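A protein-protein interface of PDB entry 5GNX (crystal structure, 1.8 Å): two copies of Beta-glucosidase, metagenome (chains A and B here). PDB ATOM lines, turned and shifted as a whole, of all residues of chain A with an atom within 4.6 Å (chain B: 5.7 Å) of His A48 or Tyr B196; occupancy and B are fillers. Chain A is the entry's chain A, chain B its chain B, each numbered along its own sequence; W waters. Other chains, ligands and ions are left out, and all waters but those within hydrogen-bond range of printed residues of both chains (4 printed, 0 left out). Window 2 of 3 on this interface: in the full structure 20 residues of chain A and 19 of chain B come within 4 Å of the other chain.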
ATOM      1  N   GLU A  40      31.836  16.626  -7.823  1.00  0.00           N
ATOM      2  CA  GLU A  40      31.372  15.555  -8.670  1.00  0.00           C
ATOM      3  C   GLU A  40      32.415  15.274  -9.758  1.00  0.00           C
ATOM      4  O   GLU A  40      32.993  16.229 -10.323  1.00  0.00           O
ATOM      5  CB  GLU A  40      30.032  15.988  -9.321  1.00  0.00           C
ATOM      6  CG  GLU A  40      29.325  14.971 -10.132  1.00  0.00           C
ATOM      7  CD  GLU A  40      27.916  15.461 -10.527  1.00  0.00           C
ATOM      8  OE1 GLU A  40      26.968  15.211  -9.761  1.00  0.00           O
ATOM      9  OE2 GLU A  40      27.746  16.036 -11.619  1.00  0.00           O
ATOM     10  N   ASP A  44      31.410   9.684 -11.165  1.00  0.00           N
ATOM     11  CA  ASP A  44      30.240   9.780 -10.352  1.00  0.00           C
ATOM     12  C   ASP A  44      28.997   9.831 -11.278  1.00  0.00           C
ATOM     13  O   ASP A  44      28.020   9.170 -11.038  1.00  0.00           O
ATOM     14  CB  ASP A  44      30.267  11.015  -9.443  1.00  0.00           C
ATOM     15  CG  ASP A  44      31.352  10.952  -8.397  1.00  0.00           C
ATOM     16  OD1 ASP A  44      31.575   9.844  -7.801  1.00  0.00           O
ATOM     17  OD2 ASP A  44      32.013  11.988  -8.140  1.00  0.00           O
ATOM     18  N   ARG A  45      29.058  10.621 -12.347  1.00  0.00           N
ATOM     19  CA  ARG A  45      27.956  10.683 -13.265  1.00  0.00           C
ATOM     20  C   ARG A  45      27.760   9.358 -14.061  1.00  0.00           C
ATOM     21  O   ARG A  45      26.661   8.846 -14.163  1.00  0.00           O
ATOM     22  CB  ARG A  45      28.168  11.790 -14.284  1.00  0.00           C
ATOM     23  CG  ARG A  45      27.943  13.188 -13.738  1.00  0.00           C
ATOM     24  CD  ARG A  45      28.286  14.201 -14.811  1.00  0.00           C
ATOM     25  NE  ARG A  45      27.981  15.582 -14.402  1.00  0.00           N
ATOM     26  CZ  ARG A  45      28.194  16.648 -15.186  1.00  0.00           C
ATOM     27  NH1 ARG A  45      28.793  16.507 -16.373  1.00  0.00           N
ATOM     28  NH2 ARG A  45      27.882  17.848 -14.744  1.00  0.00           N
ATOM     29  N   PHE A  46      28.852   8.893 -14.663  1.00  0.00           N
ATOM     30  CA  PHE A  46      28.835   7.728 -15.537  1.00  0.00           C
ATOM     31  C   PHE A  46      28.307   6.499 -14.812  1.00  0.00           C
ATOM     32  O   PHE A  46      27.461   5.767 -15.326  1.00  0.00           O
ATOM     33  CB  PHE A  46      30.264   7.473 -16.081  1.00  0.00           C
ATOM     34  CG  PHE A  46      30.346   6.447 -17.174  1.00  0.00           C
ATOM     35  CD1 PHE A  46      30.105   6.801 -18.509  1.00  0.00           C
ATOM     36  CD2 PHE A  46      30.703   5.120 -16.894  1.00  0.00           C
ATOM     37  CE1 PHE A  46      30.183   5.817 -19.529  1.00  0.00           C
ATOM     38  CE2 PHE A  46      30.806   4.154 -17.913  1.00  0.00           C
ATOM     39  CZ  PHE A  46      30.544   4.514 -19.213  1.00  0.00           C
ATOM     40  N   SER A  47      28.793   6.253 -13.584  1.00  0.00           N
ATOM     41  CA  SER A  47      28.395   5.069 -12.868  1.00  0.00           C
ATOM     42  C   SER A  47      26.923   5.113 -12.397  1.00  0.00           C
ATOM     43  O   SER A  47      26.330   4.071 -12.117  1.00  0.00           O
ATOM     44  CB  SER A  47      29.327   4.810 -11.635  1.00  0.00           C
ATOM     45  OG  SER A  47      29.032   5.761 -10.651  1.00  0.00           O
ATOM     46  N   HIS A  48      26.323   6.296 -12.346  1.00  0.00           N
ATOM     47  CA  HIS A  48      24.956   6.440 -11.944  1.00  0.00           C
ATOM     48  C   HIS A  48      24.005   6.603 -13.125  1.00  0.00           C
ATOM     49  O   HIS A  48      22.876   7.110 -12.983  1.00  0.00           O
ATOM     50  CB  HIS A  48      24.772   7.578 -10.971  1.00  0.00           C
ATOM     51  CG  HIS A  48      25.348   7.293  -9.606  1.00  0.00           C
ATOM     52  ND1 HIS A  48      24.580   6.837  -8.559  1.00  0.00           N
ATOM     53  CD2 HIS A  48      26.610   7.363  -9.134  1.00  0.00           C
ATOM     54  CE1 HIS A  48      25.346   6.649  -7.496  1.00  0.00           C
ATOM     55  NE2 HIS A  48      26.579   6.954  -7.819  1.00  0.00           N
ATOM     56  N   THR A  49      24.461   6.167 -14.271  1.00  0.00           N
ATOM     57  CA  THR A  49      23.643   6.166 -15.500  1.00  0.00           C
ATOM     58  C   THR A  49      23.363   4.688 -15.838  1.00  0.00           C
ATOM     59  O   THR A  49      24.288   3.893 -15.964  1.00  0.00           O
ATOM     60  CB  THR A  49      24.376   6.875 -16.625  1.00  0.00           C
ATOM     61  OG1 THR A  49      24.733   8.181 -16.193  1.00  0.00           O
ATOM     62  CG2 THR A  49      23.502   6.964 -17.911  1.00  0.00           C
ATOM     63  N   PRO A  50      22.081   4.327 -15.998  1.00  0.00           N
ATOM     64  CA  PRO A  50      21.753   2.913 -16.183  1.00  0.00           C
ATOM     65  C   PRO A  50      22.368   2.334 -17.434  1.00  0.00           C
ATOM     66  O   PRO A  50      22.462   3.043 -18.451  1.00  0.00           O
ATOM     67  CB  PRO A  50      20.203   2.900 -16.253  1.00  0.00           C
ATOM     68  CG  PRO A  50      19.789   4.310 -16.369  1.00  0.00           C
ATOM     69  CD  PRO A  50      20.879   5.183 -15.868  1.00  0.00           C
ATOM     70  N   THR A  58      28.614   0.753  -8.609  1.00  0.00           N
ATOM     71  CA  THR A  58      29.152   2.140  -8.604  1.00  0.00           C
ATOM     72  C   THR A  58      30.352   2.170  -7.643  1.00  0.00           C
ATOM     73  O   THR A  58      30.566   1.218  -6.848  1.00  0.00           O
ATOM     74  CB  THR A  58      28.150   3.205  -8.121  1.00  0.00           C
ATOM     75  OG1 THR A  58      28.075   3.110  -6.698  1.00  0.00           O
ATOM     76  CG2 THR A  58      26.749   2.972  -8.739  1.00  0.00           C
ATOM     77  N   ASP A  60      30.392   4.212  -5.171  1.00  0.00           N
ATOM     78  CA  ASP A  60      29.904   5.022  -4.039  1.00  0.00           C
ATOM     79  C   ASP A  60      30.528   4.545  -2.717  1.00  0.00           C
ATOM     80  O   ASP A  60      30.686   5.328  -1.784  1.00  0.00           O
ATOM     81  CB  ASP A  60      28.374   4.975  -3.907  1.00  0.00           C
ATOM     82  CG  ASP A  60      27.670   5.868  -4.888  1.00  0.00           C
ATOM     83  OD1 ASP A  60      28.328   6.469  -5.764  1.00  0.00           O
ATOM     84  OD2 ASP A  60      26.415   5.958  -4.791  1.00  0.00           O
ATOM     85  N   SER B 194      23.269  10.942 -20.676  1.00  0.00           N
ATOM     86  CA  SER B 194      23.454  11.268 -19.263  1.00  0.00           C
ATOM     87  C   SER B 194      22.291  12.124 -18.792  1.00  0.00           C
ATOM     88  O   SER B 194      22.057  13.175 -19.381  1.00  0.00           O
ATOM     89  CB  SER B 194      24.770  12.027 -19.096  1.00  0.00           C
ATOM     90  OG  SER B 194      24.908  12.558 -17.775  1.00  0.00           O
ATOM     91  N   ALA B 195      21.622  11.732 -17.730  1.00  0.00           N
ATOM     92  CA  ALA B 195      20.593  12.620 -17.123  1.00  0.00           C
ATOM     93  C   ALA B 195      21.239  13.835 -16.526  1.00  0.00           C
ATOM     94  O   ALA B 195      20.669  14.925 -16.534  1.00  0.00           O
ATOM     95  CB  ALA B 195      19.753  11.874 -16.066  1.00  0.00           C
ATOM     96  N   TYR B 196      22.441  13.663 -15.908  1.00  0.00           N
ATOM     97  CA  TYR B 196      23.128  14.790 -15.329  1.00  0.00           C
ATOM     98  C   TYR B 196      23.362  15.881 -16.371  1.00  0.00           C
ATOM     99  O   TYR B 196      23.127  17.064 -16.118  1.00  0.00           O
ATOM    100  CB  TYR B 196      24.493  14.351 -14.746  1.00  0.00           C
ATOM    101  CG  TYR B 196      24.294  13.416 -13.581  1.00  0.00           C
ATOM    102  CD1 TYR B 196      24.151  12.065 -13.782  1.00  0.00           C
ATOM    103  CD2 TYR B 196      24.247  13.903 -12.280  1.00  0.00           C
ATOM    104  CE1 TYR B 196      23.956  11.180 -12.714  1.00  0.00           C
ATOM    105  CE2 TYR B 196      24.035  13.045 -11.206  1.00  0.00           C
ATOM    106  CZ  TYR B 196      23.903  11.693 -11.424  1.00  0.00           C
ATOM    107  OH  TYR B 196      23.678  10.831 -10.359  1.00  0.00           O
ATOM    108  N   GLU B 197      23.870  15.475 -17.544  1.00  0.00           N
ATOM    109  CA  GLU B 197      24.097  16.414 -18.600  1.00  0.00           C
ATOM    110  C   GLU B 197      22.826  16.999 -19.176  1.00  0.00           C
ATOM    111  O   GLU B 197      22.791  18.191 -19.513  1.00  0.00           O
ATOM    112  CB  GLU B 197      24.891  15.774 -19.726  1.00  0.00           C
ATOM    113  CG  GLU B 197      26.316  15.381 -19.309  1.00  0.00           C
ATOM    114  CD  GLU B 197      27.153  14.890 -20.474  1.00  0.00           C
ATOM    115  OE1 GLU B 197      26.811  15.195 -21.650  1.00  0.00           O
ATOM    116  OE2 GLU B 197      28.203  14.235 -20.216  1.00  0.00           O
ATOM    117  N   ALA B 198      21.813  16.164 -19.312  1.00  0.00           N
ATOM    118  CA  ALA B 198      20.537  16.614 -19.911  1.00  0.00           C
ATOM    119  C   ALA B 198      19.927  17.769 -19.114  1.00  0.00           C
ATOM    120  O   ALA B 198      19.398  18.721 -19.671  1.00  0.00           O
ATOM    121  CB  ALA B 198      19.552  15.455 -20.016  1.00  0.00           C
ATOM    122  N   VAL B 199      20.019  17.678 -17.802  1.00  0.00           N
ATOM    123  CA  VAL B 199      19.448  18.702 -16.935  1.00  0.00           C
ATOM    124  C   VAL B 199      20.143  20.012 -17.142  1.00  0.00           C
ATOM    125  O   VAL B 199      19.519  21.085 -17.226  1.00  0.00           O
ATOM    126  CB  VAL B 199      19.526  18.283 -15.414  1.00  0.00           C
ATOM    127  CG1 VAL B 199      19.202  19.491 -14.494  1.00  0.00           C
ATOM    128  CG2 VAL B 199      18.564  17.101 -15.184  1.00  0.00           C
ATOM    129  N   ILE B 200      21.466  19.952 -17.195  1.00  0.00           N
ATOM    130  CA  ILE B 200      22.267  21.146 -17.412  1.00  0.00           C
ATOM    131  C   ILE B 200      22.065  21.703 -18.816  1.00  0.00           C
ATOM    132  O   ILE B 200      21.904  22.939 -18.998  1.00  0.00           O
ATOM    133  CB  ILE B 200      23.755  20.816 -17.145  1.00  0.00           C
ATOM    134  CG1 ILE B 200      23.960  20.552 -15.659  1.00  0.00           C
ATOM    135  CG2 ILE B 200      24.671  21.948 -17.676  1.00  0.00           C
ATOM    136  CD1 ILE B 200      25.316  19.851 -15.335  1.00  0.00           C
ATOM    137  N   ALA B 201      22.072  20.841 -19.826  1.00  0.00           N
ATOM    138  CA  ALA B 201      21.993  21.316 -21.215  1.00  0.00           C
ATOM    139  C   ALA B 201      20.634  21.998 -21.460  1.00  0.00           C
ATOM    140  O   ALA B 201      20.573  23.080 -22.077  1.00  0.00           O
ATOM    141  CB  ALA B 201      22.196  20.134 -22.207  1.00  0.00           C
ATOM    142  N   ALA B 276      18.599  12.073  -8.732  1.00  0.00           N
ATOM    143  CA  ALA B 276      19.762  12.738  -8.158  1.00  0.00           C
ATOM    144  C   ALA B 276      20.499  13.576  -9.203  1.00  0.00           C
ATOM    145  O   ALA B 276      21.411  14.353  -8.849  1.00  0.00           O
ATOM    146  CB  ALA B 276      20.705  11.693  -7.559  1.00  0.00           C
ATOM    147  N   ALA B 277      20.118  13.453 -10.480  1.00  0.00           N
ATOM    148  CA  ALA B 277      20.651  14.304 -11.525  1.00  0.00           C
ATOM    149  C   ALA B 277      20.002  15.684 -11.575  1.00  0.00           C
ATOM    150  O   ALA B 277      20.558  16.610 -12.183  1.00  0.00           O
ATOM    151  CB  ALA B 277      20.491  13.641 -12.926  1.00  0.00           C
ATOM    152  N   ARG B 279      18.960  19.414 -10.600  1.00  0.00           N
ATOM    153  CA  ARG B 279      19.764  20.516 -10.043  1.00  0.00           C
ATOM    154  C   ARG B 279      18.927  21.744  -9.928  1.00  0.00           C
ATOM    155  O   ARG B 279      17.951  21.913 -10.665  1.00  0.00           O
ATOM    156  CB  ARG B 279      21.007  20.835 -10.935  1.00  0.00           C
ATOM    157  CG  ARG B 279      22.059  19.774 -11.015  1.00  0.00           C
ATOM    158  CD  ARG B 279      22.827  19.588  -9.682  1.00  0.00           C
ATOM    159  NE  ARG B 279      23.866  18.515  -9.743  1.00  0.00           N
ATOM    160  CZ  ARG B 279      23.649  17.212  -9.523  1.00  0.00           C
ATOM    161  NH1 ARG B 279      22.451  16.785  -9.235  1.00  0.00           N
ATOM    162  NH2 ARG B 279      24.652  16.336  -9.593  1.00  0.00           N
HETATM  163  O   HOH W   1      26.206  10.600 -16.838  1.00  0.00           O
HETATM  164  O   HOH W   2      25.832  17.554 -12.579  1.00  0.00           O
HETATM  165  O   HOH W   3      22.433   9.816 -15.840  1.00  0.00           O
HETATM  166  O   HOH W   4      29.985  14.029 -17.880  1.00  0.00           O
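Water W1 lies within hydrogen-bond range of OG of Ser B194 (2.5 Å), OG1 of Thr A49 (2.9 Å) and O of Arg A45 (3.2 Å).
Water W2 lies within hydrogen-bond range of OE2 of Glu A40 (2.6 Å), NH2 of Arg A45 (3.0 Å) and NH2 of Arg B279 (3.4 Å).
Water W3 bridges N of Ala B195 and OG1 of Thr A49.
Water W4 lies within hydrogen-bond range of the side-chain carboxylate of Glu B197 (2.9 Å) and the guanidinium group of Arg A45 (3.1 Å).
The guanidinium group (NH2) of Arg B279 is in salt-bridge range of the side-chain carboxylate (OE1) of Glu A40 (2.6 Å).
NH1 of Arg B279 lies within hydrogen-bond range of O of Ala B276 (2.7 Å).
The backbone carbonyl oxygen (O) of Arg A45 sits at hydrogen-bond distance from the side-chain hydroxyl (OG1) of Thr A49 (2.9 Å).
A ring nitrogen (NE2) of His A48 is in hydrogen-bond range of the side-chain carboxylate (OD1) of Asp A60 (2.7 Å).
The side-chain carboxylate (OE2) of Glu A40 is in salt-bridge range of the guanidinium group (NE) of Arg A45, at 2.8 Å.
OG of Ser B194 lies close to N of Tyr B196 (3.3 Å).
Of the printed residues of chain B, Glu A40 touches Tyr B196 (3.9 Å) and Arg B279 (2.6 Å).
Of chain B, only Tyr B196 comes within 4 Å of His A48.
Thr A49 touches none of the printed residues of chain B.
Of chain A, only Glu A40, Arg A45 and His A48 come within 4 Å of Tyr B196.
Printed residues of chain A within 4 Å of Ile B200: Arg A45.
Ala B201 touches none of the printed residues of chain A.
Of the printed residues of chain A, Arg B279 touches Glu A40 (2.6 Å).
The nearest printed residue of chain A that does not touch Tyr B196 is Thr A49 (4.6 Å).
Tyr B196 touches Glu A40 (CE2 to OE1, 3.9 Å).
Tyr B196 touches Arg A45 (CG to CG, 3.7 Å).
Arg A45 touches Ile B200.
His A48 touches Tyr B196 (CB to OH, 3.5 Å).
Hydrophobic or aromatic side chains of chain A that line the printed part of chain B: His A48.
Among the printed residues, 5 pairs touch across the chains.
No position is printed for both chains.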
